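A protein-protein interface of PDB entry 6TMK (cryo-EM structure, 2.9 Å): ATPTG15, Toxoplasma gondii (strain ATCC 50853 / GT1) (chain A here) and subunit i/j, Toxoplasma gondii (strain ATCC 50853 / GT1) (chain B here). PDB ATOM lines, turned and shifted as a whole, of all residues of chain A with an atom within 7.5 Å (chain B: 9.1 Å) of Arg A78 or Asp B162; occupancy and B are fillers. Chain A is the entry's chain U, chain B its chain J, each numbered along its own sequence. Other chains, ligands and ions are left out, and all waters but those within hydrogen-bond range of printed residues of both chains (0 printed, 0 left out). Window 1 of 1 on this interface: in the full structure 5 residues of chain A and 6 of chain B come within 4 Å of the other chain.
Ser A77 touches none of the printed residues of chain B. Arg A78 touches five residues of chain B. Of chain B, only Tyr B156 (3.5 Å) and Asp B162 (2.5 Å) come within 4 Å of Tyr A81. Of the printed residues of chain B, Ala A82 touches Tyr B156 (3.2 Å). Of the printed residues of chain B, Gln A85 touches Tyr B156, Asp B162 and His B163. Of the printed residues of chain A, Tyr B156 touches Arg A78 (2.9 Å), Tyr A81 (3.5 Å), Ala A82 (3.2 Å) and Gln A85 (2.5 Å). Printed residues of chain A within 4 Å of Cys B157: Leu A75 (3.8 Å) and Arg A78 (3.95 Å). Printed residues of chain A within 4 Å of Leu B161: Arg A78 (3.4 Å). The nearest residue of chain B that does not touch Arg A78 is Arg B155 (5.4 Å). The nearest residue of chain A that does not touch Asp B162 is His A89 (6.1 Å).
O of Leu B161 lies within hydrogen-bond range of NH2 of Arg A78 (3.4 Å). OD1 of Asp B162 lies within salt-bridge range of NH2 of Arg A78. The backbone carbonyl oxygen (O) of Tyr B156 is in hydrogen-bond range of the guanidinium group (NE) of Arg A78 (2.9 Å). OE1 of Gln A85 lies within hydrogen-bond range of OH of Tyr B156, 2.5 Å away. NE2 of Gln A85 is in hydrogen-bond range of O of Asp B162 (3.0 Å). The side-chain carboxylate (OD2) of Asp B162 is in hydrogen-bond range of the side-chain hydroxyl (OH) of Tyr A81 (2.5 Å).
A ring nitrogen (ND1) of His A89 lies within hydrogen-bond range of the backbone carbonyl oxygen of Gln A85 (3.5 Å). O of Arg B155 is in hydrogen-bond range of N of Leu B161, at 3.1 Å. The backbone carbonyl oxygen (O) of Arg B155 lies within hydrogen-bond range of the backbone NH (N) of Gly B160 (3.4 Å).
Leu A75 touches Cys B157 (CD1 to CB, 3.8 Å). Arg A78 touches Cys B157. Arg A78 touches Gly B160 (NH2 to C, 3.5 Å). Tyr B156 touches Tyr A81 (OH to CD2, 3.5 Å). CA of Ala A82 touches OH of Tyr B156 (3.2 Å). CE1 of His B163 touches NE2 of Gln A85, 3.6 Å away.
Hydrophobic or aromatic side chains of chain B within 4 Å of the printed part of chain A: Tyr B156 and His B163. Along chain B the printed residues that touch a printed residue of chain A span positions 156 to 163. Of the 15 printed residues of chain A, 5 touch a printed residue of chain B. Among the printed residues, 12 pairs touch across the chains. Among the printed residues, Asp or Glu carboxylates within 4 Å of a Lys or Arg side-chain nitrogen of the other chain: Arg A78 with Asp B162 (2.6 Å).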
ATOM      1  N   SER A  72     -11.820  -6.475 -16.910  1.00  0.00           N
ATOM      2  CA  SER A  72     -13.119  -6.091 -16.375  1.00  0.00           C
ATOM      3  C   SER A  72     -13.370  -6.762 -15.035  1.00  0.00           C
ATOM      4  O   SER A  72     -13.789  -6.115 -14.071  1.00  0.00           O
ATOM      5  CB  SER A  72     -14.214  -6.454 -17.374  1.00  0.00           C
ATOM      6  OG  SER A  72     -13.965  -5.854 -18.631  1.00  0.00           O
ATOM      7  N   VAL A  73     -13.109  -8.065 -14.956  1.00  0.00           N
ATOM      8  CA  VAL A  73     -13.336  -8.807 -13.720  1.00  0.00           C
ATOM      9  C   VAL A  73     -12.404  -8.306 -12.628  1.00  0.00           C
ATOM     10  O   VAL A  73     -12.818  -8.079 -11.482  1.00  0.00           O
ATOM     11  CB  VAL A  73     -13.150 -10.313 -13.969  1.00  0.00           C
ATOM     12  CG1 VAL A  73     -13.044 -11.069 -12.667  1.00  0.00           C
ATOM     13  CG2 VAL A  73     -14.286 -10.838 -14.791  1.00  0.00           C
ATOM     14  N   ALA A  74     -11.125  -8.143 -12.965  1.00  0.00           N
ATOM     15  CA  ALA A  74     -10.168  -7.677 -11.970  1.00  0.00           C
ATOM     16  C   ALA A  74     -10.556  -6.302 -11.443  1.00  0.00           C
ATOM     17  O   ALA A  74     -10.497  -6.047 -10.233  1.00  0.00           O
ATOM     18  CB  ALA A  74      -8.774  -7.654 -12.575  1.00  0.00           C
ATOM     19  N   LEU A  75     -10.973  -5.411 -12.338  1.00  0.00           N
ATOM     20  CA  LEU A  75     -11.344  -4.063 -11.946  1.00  0.00           C
ATOM     21  C   LEU A  75     -12.618  -4.060 -11.118  1.00  0.00           C
ATOM     22  O   LEU A  75     -12.751  -3.270 -10.182  1.00  0.00           O
ATOM     23  CB  LEU A  75     -11.497  -3.202 -13.192  1.00  0.00           C
ATOM     24  CG  LEU A  75     -11.778  -1.721 -12.988  1.00  0.00           C
ATOM     25  CD1 LEU A  75     -10.584  -1.027 -12.385  1.00  0.00           C
ATOM     26  CD2 LEU A  75     -12.149  -1.113 -14.308  1.00  0.00           C
ATOM     27  N   GLN A  76     -13.576  -4.915 -11.462  1.00  0.00           N
ATOM     28  CA  GLN A  76     -14.797  -5.023 -10.676  1.00  0.00           C
ATOM     29  C   GLN A  76     -14.484  -5.467  -9.254  1.00  0.00           C
ATOM     30  O   GLN A  76     -15.008  -4.911  -8.278  1.00  0.00           O
ATOM     31  CB  GLN A  76     -15.748  -6.002 -11.354  1.00  0.00           C
ATOM     32  CG  GLN A  76     -16.476  -5.425 -12.538  1.00  0.00           C
ATOM     33  CD  GLN A  76     -17.300  -6.459 -13.270  1.00  0.00           C
ATOM     34  OE1 GLN A  76     -17.562  -7.541 -12.750  1.00  0.00           O
ATOM     35  NE2 GLN A  76     -17.699  -6.137 -14.490  1.00  0.00           N
ATOM     36  N   SER A  77     -13.629  -6.480  -9.120  1.00  0.00           N
ATOM     37  CA  SER A  77     -13.207  -6.930  -7.801  1.00  0.00           C
ATOM     38  C   SER A  77     -12.547  -5.796  -7.031  1.00  0.00           C
ATOM     39  O   SER A  77     -12.853  -5.557  -5.854  1.00  0.00           O
ATOM     40  CB  SER A  77     -12.259  -8.119  -7.952  1.00  0.00           C
ATOM     41  OG  SER A  77     -12.135  -8.851  -6.751  1.00  0.00           O
ATOM     42  N   ARG A  78     -11.635  -5.082  -7.690  1.00  0.00           N
ATOM     43  CA  ARG A  78     -10.931  -3.994  -7.033  1.00  0.00           C
ATOM     44  C   ARG A  78     -11.875  -2.866  -6.637  1.00  0.00           C
ATOM     45  O   ARG A  78     -11.679  -2.227  -5.598  1.00  0.00           O
ATOM     46  CB  ARG A  78      -9.830  -3.497  -7.962  1.00  0.00           C
ATOM     47  CG  ARG A  78      -8.870  -2.521  -7.365  1.00  0.00           C
ATOM     48  CD  ARG A  78      -8.176  -3.057  -6.162  1.00  0.00           C
ATOM     49  NE  ARG A  78      -7.208  -2.105  -5.648  1.00  0.00           N
ATOM     50  CZ  ARG A  78      -6.699  -2.155  -4.430  1.00  0.00           C
ATOM     51  NH1 ARG A  78      -7.044  -3.111  -3.603  1.00  0.00           N
ATOM     52  NH2 ARG A  78      -5.837  -1.249  -4.044  1.00  0.00           N
ATOM     53  N   LEU A  79     -12.928  -2.636  -7.417  1.00  0.00           N
ATOM     54  CA  LEU A  79     -13.870  -1.574  -7.093  1.00  0.00           C
ATOM     55  C   LEU A  79     -14.764  -1.962  -5.924  1.00  0.00           C
ATOM     56  O   LEU A  79     -15.118  -1.114  -5.097  1.00  0.00           O
ATOM     57  CB  LEU A  79     -14.698  -1.234  -8.325  1.00  0.00           C
ATOM     58  CG  LEU A  79     -13.924  -0.516  -9.428  1.00  0.00           C
ATOM     59  CD1 LEU A  79     -14.723  -0.470 -10.700  1.00  0.00           C
ATOM     60  CD2 LEU A  79     -13.521   0.865  -9.017  1.00  0.00           C
ATOM     61  N   ARG A  80     -15.139  -3.235  -5.834  1.00  0.00           N
ATOM     62  CA  ARG A  80     -15.850  -3.709  -4.651  1.00  0.00           C
ATOM     63  C   ARG A  80     -14.996  -3.562  -3.396  1.00  0.00           C
ATOM     64  O   ARG A  80     -15.480  -3.131  -2.336  1.00  0.00           O
ATOM     65  CB  ARG A  80     -16.270  -5.158  -4.864  1.00  0.00           C
ATOM     66  CG  ARG A  80     -17.323  -5.325  -5.921  1.00  0.00           C
ATOM     67  CD  ARG A  80     -17.816  -6.741  -5.994  1.00  0.00           C
ATOM     68  NE  ARG A  80     -17.210  -7.490  -7.091  1.00  0.00           N
ATOM     69  CZ  ARG A  80     -16.542  -8.629  -6.960  1.00  0.00           C
ATOM     70  NH1 ARG A  80     -16.349  -9.187  -5.777  1.00  0.00           N
ATOM     71  NH2 ARG A  80     -16.055  -9.210  -8.035  1.00  0.00           N
ATOM     72  N   TYR A  81     -13.719  -3.924  -3.503  1.00  0.00           N
ATOM     73  CA  TYR A  81     -12.772  -3.687  -2.420  1.00  0.00           C
ATOM     74  C   TYR A  81     -12.742  -2.213  -2.032  1.00  0.00           C
ATOM     75  O   TYR A  81     -12.749  -1.866  -0.842  1.00  0.00           O
ATOM     76  CB  TYR A  81     -11.398  -4.177  -2.867  1.00  0.00           C
ATOM     77  CG  TYR A  81     -10.300  -4.131  -1.844  1.00  0.00           C
ATOM     78  CD1 TYR A  81     -10.002  -5.243  -1.089  1.00  0.00           C
ATOM     79  CD2 TYR A  81      -9.539  -2.997  -1.657  1.00  0.00           C
ATOM     80  CE1 TYR A  81      -8.999  -5.223  -0.174  1.00  0.00           C
ATOM     81  CE2 TYR A  81      -8.538  -2.970  -0.741  1.00  0.00           C
ATOM     82  CZ  TYR A  81      -8.267  -4.086  -0.001  1.00  0.00           C
ATOM     83  OH  TYR A  81      -7.255  -4.058   0.921  1.00  0.00           O
ATOM     84  N   ALA A  82     -12.717  -1.329  -3.030  1.00  0.00           N
ATOM     85  CA  ALA A  82     -12.700   0.101  -2.765  1.00  0.00           C
ATOM     86  C   ALA A  82     -13.963   0.545  -2.045  1.00  0.00           C
ATOM     87  O   ALA A  82     -13.915   1.427  -1.183  1.00  0.00           O
ATOM     88  CB  ALA A  82     -12.536   0.858  -4.075  1.00  0.00           C
ATOM     89  N   GLU A  83     -15.107  -0.032  -2.403  1.00  0.00           N
ATOM     90  CA  GLU A  83     -16.351   0.312  -1.726  1.00  0.00           C
ATOM     91  C   GLU A  83     -16.290  -0.056  -0.251  1.00  0.00           C
ATOM     92  O   GLU A  83     -16.673   0.735   0.623  1.00  0.00           O
ATOM     93  CB  GLU A  83     -17.515  -0.396  -2.401  1.00  0.00           C
ATOM     94  CG  GLU A  83     -18.846   0.246  -2.144  1.00  0.00           C
ATOM     95  CD  GLU A  83     -19.996  -0.665  -2.483  1.00  0.00           C
ATOM     96  OE1 GLU A  83     -19.773  -1.660  -3.201  1.00  0.00           O
ATOM     97  OE2 GLU A  83     -21.125  -0.392  -2.030  1.00  0.00           O
ATOM     98  N   LYS A  84     -15.830  -1.272   0.044  1.00  0.00           N
ATOM     99  CA  LYS A  84     -15.671  -1.682   1.436  1.00  0.00           C
ATOM    100  C   LYS A  84     -14.763  -0.719   2.190  1.00  0.00           C
ATOM    101  O   LYS A  84     -15.069  -0.298   3.313  1.00  0.00           O
ATOM    102  CB  LYS A  84     -15.123  -3.100   1.489  1.00  0.00           C
ATOM    103  CG  LYS A  84     -16.107  -4.135   1.084  1.00  0.00           C
ATOM    104  CD  LYS A  84     -15.500  -5.505   1.070  1.00  0.00           C
ATOM    105  CE  LYS A  84     -16.474  -6.524   0.526  1.00  0.00           C
ATOM    106  NZ  LYS A  84     -16.288  -6.759  -0.931  1.00  0.00           N
ATOM    107  N   GLN A  85     -13.637  -0.360   1.576  1.00  0.00           N
ATOM    108  CA  GLN A  85     -12.688   0.556   2.195  1.00  0.00           C
ATOM    109  C   GLN A  85     -13.331   1.909   2.477  1.00  0.00           C
ATOM    110  O   GLN A  85     -13.170   2.483   3.565  1.00  0.00           O
ATOM    111  CB  GLN A  85     -11.487   0.694   1.271  1.00  0.00           C
ATOM    112  CG  GLN A  85     -10.439   1.647   1.701  1.00  0.00           C
ATOM    113  CD  GLN A  85      -9.225   1.564   0.822  1.00  0.00           C
ATOM    114  OE1 GLN A  85      -9.206   0.827  -0.159  1.00  0.00           O
ATOM    115  NE2 GLN A  85      -8.209   2.319   1.160  1.00  0.00           N
ATOM    116  N   HIS A  89     -13.887   3.681   6.228  1.00  0.00           N
ATOM    117  CA  HIS A  89     -13.354   4.986   6.600  1.00  0.00           C
ATOM    118  C   HIS A  89     -14.462   5.949   6.998  1.00  0.00           C
ATOM    119  O   HIS A  89     -14.318   6.721   7.957  1.00  0.00           O
ATOM    120  CB  HIS A  89     -12.539   5.551   5.442  1.00  0.00           C
ATOM    121  CG  HIS A  89     -11.145   5.023   5.371  1.00  0.00           C
ATOM    122  ND1 HIS A  89     -10.537   4.689   4.182  1.00  0.00           N
ATOM    123  CD2 HIS A  89     -10.225   4.804   6.339  1.00  0.00           C
ATOM    124  CE1 HIS A  89      -9.312   4.263   4.422  1.00  0.00           C
ATOM    125  NE2 HIS A  89      -9.097   4.326   5.723  1.00  0.00           N
ATOM    126  N   TYR B 152      -4.469   8.610  -9.270  1.00  0.00           N
ATOM    127  CA  TYR B 152      -5.104   7.794  -8.245  1.00  0.00           C
ATOM    128  C   TYR B 152      -5.517   6.442  -8.806  1.00  0.00           C
ATOM    129  O   TYR B 152      -5.287   5.402  -8.183  1.00  0.00           O
ATOM    130  CB  TYR B 152      -6.307   8.534  -7.664  1.00  0.00           C
ATOM    131  CG  TYR B 152      -6.831   7.937  -6.384  1.00  0.00           C
ATOM    132  CD1 TYR B 152      -6.448   8.433  -5.155  1.00  0.00           C
ATOM    133  CD2 TYR B 152      -7.722   6.886  -6.408  1.00  0.00           C
ATOM    134  CE1 TYR B 152      -6.926   7.893  -3.993  1.00  0.00           C
ATOM    135  CE2 TYR B 152      -8.203   6.338  -5.249  1.00  0.00           C
ATOM    136  CZ  TYR B 152      -7.807   6.845  -4.046  1.00  0.00           C
ATOM    137  OH  TYR B 152      -8.297   6.290  -2.892  1.00  0.00           O
ATOM    138  N   GLU B 153      -6.145   6.444  -9.981  1.00  0.00           N
ATOM    139  CA  GLU B 153      -6.540   5.206 -10.638  1.00  0.00           C
ATOM    140  C   GLU B 153      -5.332   4.323 -10.907  1.00  0.00           C
ATOM    141  O   GLU B 153      -5.319   3.142 -10.553  1.00  0.00           O
ATOM    142  CB  GLU B 153      -7.279   5.529 -11.930  1.00  0.00           C
ATOM    143  CG  GLU B 153      -7.727   4.329 -12.725  1.00  0.00           C
ATOM    144  CD  GLU B 153      -8.113   4.695 -14.135  1.00  0.00           C
ATOM    145  OE1 GLU B 153      -8.522   5.853 -14.349  1.00  0.00           O
ATOM    146  OE2 GLU B 153      -7.998   3.835 -15.034  1.00  0.00           O
ATOM    147  N   ALA B 154      -4.314   4.874 -11.559  1.00  0.00           N
ATOM    148  CA  ALA B 154      -3.174   4.071 -11.964  1.00  0.00           C
ATOM    149  C   ALA B 154      -2.485   3.447 -10.764  1.00  0.00           C
ATOM    150  O   ALA B 154      -1.908   2.362 -10.877  1.00  0.00           O
ATOM    151  CB  ALA B 154      -2.192   4.925 -12.758  1.00  0.00           C
ATOM    152  N   ARG B 155      -2.523   4.110  -9.613  1.00  0.00           N
ATOM    153  CA  ARG B 155      -1.911   3.538  -8.423  1.00  0.00           C
ATOM    154  C   ARG B 155      -2.831   2.587  -7.668  1.00  0.00           C
ATOM    155  O   ARG B 155      -2.341   1.630  -7.061  1.00  0.00           O
ATOM    156  CB  ARG B 155      -1.450   4.649  -7.487  1.00  0.00           C
ATOM    157  CG  ARG B 155      -0.274   5.413  -8.002  1.00  0.00           C
ATOM    158  CD  ARG B 155       0.173   6.469  -7.045  1.00  0.00           C
ATOM    159  NE  ARG B 155       1.231   7.296  -7.605  1.00  0.00           N
ATOM    160  CZ  ARG B 155       1.427   8.570  -7.299  1.00  0.00           C
ATOM    161  NH1 ARG B 155       0.648   9.179  -6.428  1.00  0.00           N
ATOM    162  NH2 ARG B 155       2.406   9.240  -7.868  1.00  0.00           N
ATOM    163  N   TYR B 156      -4.142   2.814  -7.679  1.00  0.00           N
ATOM    164  CA  TYR B 156      -5.067   2.008  -6.895  1.00  0.00           C
ATOM    165  C   TYR B 156      -5.501   0.751  -7.637  1.00  0.00           C
ATOM    166  O   TYR B 156      -5.452  -0.350  -7.084  1.00  0.00           O
ATOM    167  CB  TYR B 156      -6.307   2.831  -6.528  1.00  0.00           C
ATOM    168  CG  TYR B 156      -7.176   2.184  -5.480  1.00  0.00           C
ATOM    169  CD1 TYR B 156      -6.988   2.442  -4.141  1.00  0.00           C
ATOM    170  CD2 TYR B 156      -8.176   1.298  -5.838  1.00  0.00           C
ATOM    171  CE1 TYR B 156      -7.767   1.847  -3.192  1.00  0.00           C
ATOM    172  CE2 TYR B 156      -8.957   0.695  -4.894  1.00  0.00           C
ATOM    173  CZ  TYR B 156      -8.754   0.971  -3.570  1.00  0.00           C
ATOM    174  OH  TYR B 156      -9.543   0.362  -2.628  1.00  0.00           O
ATOM    175  N   CYS B 157      -5.934   0.906  -8.881  1.00  0.00           N
ATOM    176  CA  CYS B 157      -6.644  -0.137  -9.597  1.00  0.00           C
ATOM    177  C   CYS B 157      -5.740  -1.010 -10.454  1.00  0.00           C
ATOM    178  O   CYS B 157      -6.199  -2.042 -10.951  1.00  0.00           O
ATOM    179  CB  CYS B 157      -7.721   0.496 -10.476  1.00  0.00           C
ATOM    180  SG  CYS B 157      -8.746   1.693  -9.612  1.00  0.00           S
ATOM    181  N   TYR B 158      -4.476  -0.636 -10.634  1.00  0.00           N
ATOM    182  CA  TYR B 158      -3.582  -1.366 -11.514  1.00  0.00           C
ATOM    183  C   TYR B 158      -2.244  -1.684 -10.878  1.00  0.00           C
ATOM    184  O   TYR B 158      -1.496  -2.496 -11.432  1.00  0.00           O
ATOM    185  CB  TYR B 158      -3.363  -0.590 -12.821  1.00  0.00           C
ATOM    186  CG  TYR B 158      -4.620  -0.484 -13.635  1.00  0.00           C
ATOM    187  CD1 TYR B 158      -5.122  -1.582 -14.302  1.00  0.00           C
ATOM    188  CD2 TYR B 158      -5.318   0.703 -13.722  1.00  0.00           C
ATOM    189  CE1 TYR B 158      -6.273  -1.501 -15.031  1.00  0.00           C
ATOM    190  CE2 TYR B 158      -6.471   0.793 -14.448  1.00  0.00           C
ATOM    191  CZ  TYR B 158      -6.947  -0.312 -15.103  1.00  0.00           C
ATOM    192  OH  TYR B 158      -8.105  -0.233 -15.839  1.00  0.00           O
ATOM    193  N   ARG B 159      -1.925  -1.083  -9.738  1.00  0.00           N
ATOM    194  CA  ARG B 159      -0.729  -1.412  -8.983  1.00  0.00           C
ATOM    195  C   ARG B 159      -1.019  -2.012  -7.619  1.00  0.00           C
ATOM    196  O   ARG B 159      -0.138  -2.668  -7.057  1.00  0.00           O
ATOM    197  CB  ARG B 159       0.137  -0.162  -8.800  1.00  0.00           C
ATOM    198  CG  ARG B 159       1.585  -0.437  -8.554  1.00  0.00           C
ATOM    199  CD  ARG B 159       2.289   0.830  -8.202  1.00  0.00           C
ATOM    200  NE  ARG B 159       2.355   1.732  -9.337  1.00  0.00           N
ATOM    201  CZ  ARG B 159       2.884   2.945  -9.283  1.00  0.00           C
ATOM    202  NH1 ARG B 159       3.388   3.403  -8.148  1.00  0.00           N
ATOM    203  NH2 ARG B 159       2.908   3.699 -10.368  1.00  0.00           N
ATOM    204  N   GLY B 160      -2.204  -1.794  -7.069  1.00  0.00           N
ATOM    205  CA  GLY B 160      -2.620  -2.443  -5.850  1.00  0.00           C
ATOM    206  C   GLY B 160      -2.414  -1.646  -4.588  1.00  0.00           C
ATOM    207  O   GLY B 160      -2.421  -2.237  -3.503  1.00  0.00           O
ATOM    208  N   LEU B 161      -2.234  -0.337  -4.689  1.00  0.00           N
ATOM    209  CA  LEU B 161      -2.014   0.505  -3.526  1.00  0.00           C
ATOM    210  C   LEU B 161      -3.353   0.977  -2.982  1.00  0.00           C
ATOM    211  O   LEU B 161      -4.112   1.648  -3.686  1.00  0.00           O
ATOM    212  CB  LEU B 161      -1.143   1.701  -3.894  1.00  0.00           C
ATOM    213  CG  LEU B 161       0.180   1.394  -4.587  1.00  0.00           C
ATOM    214  CD1 LEU B 161       0.911   2.673  -4.858  1.00  0.00           C
ATOM    215  CD2 LEU B 161       1.026   0.475  -3.751  1.00  0.00           C
ATOM    216  N   ASP B 162      -3.629   0.644  -1.726  1.00  0.00           N
ATOM    217  CA  ASP B 162      -4.866   1.067  -1.093  1.00  0.00           C
ATOM    218  C   ASP B 162      -4.826   2.532  -0.693  1.00  0.00           C
ATOM    219  O   ASP B 162      -5.883   3.153  -0.548  1.00  0.00           O
ATOM    220  CB  ASP B 162      -5.155   0.195   0.124  1.00  0.00           C
ATOM    221  CG  ASP B 162      -5.692  -1.161  -0.248  1.00  0.00           C
ATOM    222  OD1 ASP B 162      -5.650  -1.512  -1.442  1.00  0.00           O
ATOM    223  OD2 ASP B 162      -6.145  -1.886   0.656  1.00  0.00           O
ATOM    224  N   HIS B 163      -3.633   3.088  -0.520  1.00  0.00           N
ATOM    225  CA  HIS B 163      -3.438   4.465  -0.078  1.00  0.00           C
ATOM    226  C   HIS B 163      -2.496   5.150  -1.053  1.00  0.00           C
ATOM    227  O   HIS B 163      -1.305   5.338  -0.768  1.00  0.00           O
ATOM    228  CB  HIS B 163      -2.921   4.496   1.356  1.00  0.00           C
ATOM    229  CG  HIS B 163      -3.738   3.673   2.294  1.00  0.00           C
ATOM    230  ND1 HIS B 163      -5.028   4.008   2.638  1.00  0.00           N
ATOM    231  CD2 HIS B 163      -3.468   2.512   2.931  1.00  0.00           C
ATOM    232  CE1 HIS B 163      -5.509   3.098   3.463  1.00  0.00           C
ATOM    233  NE2 HIS B 163      -4.583   2.178   3.655  1.00  0.00           N
ATOM    234  N   PRO B 164      -2.999   5.539  -2.223  1.00  0.00           N
ATOM    235  CA  PRO B 164      -2.110   6.053  -3.270  1.00  0.00           C
ATOM    236  C   PRO B 164      -1.584   7.445  -2.991  1.00  0.00           C
ATOM    237  O   PRO B 164      -0.477   7.773  -3.427  1.00  0.00           O
ATOM    238  CB  PRO B 164      -2.996   6.025  -4.523  1.00  0.00           C
ATOM    239  CG  PRO B 164      -4.265   5.394  -4.113  1.00  0.00           C
ATOM    240  CD  PRO B 164      -4.394   5.534  -2.668  1.00  0.00           C
ATOM    241  N   PHE B 165      -2.352   8.277  -2.301  1.00  0.00           N
ATOM    242  CA  PHE B 165      -2.045   9.686  -2.131  1.00  0.00           C
ATOM    243  C   PHE B 165      -1.462   9.926  -0.751  1.00  0.00           C
ATOM    244  O   PHE B 165      -2.050   9.527   0.259  1.00  0.00           O
ATOM    245  CB  PHE B 165      -3.296  10.542  -2.328  1.00  0.00           C
ATOM    246  CG  PHE B 165      -3.573  10.904  -3.753  1.00  0.00           C
ATOM    247  CD1 PHE B 165      -2.881  10.313  -4.785  1.00  0.00           C
ATOM    248  CD2 PHE B 165      -4.545  11.830  -4.062  1.00  0.00           C
ATOM    249  CE1 PHE B 165      -3.136  10.642  -6.079  1.00  0.00           C
ATOM    250  CE2 PHE B 165      -4.807  12.158  -5.365  1.00  0.00           C
ATOM    251  CZ  PHE B 165      -4.104  11.561  -6.374  1.00  0.00           C
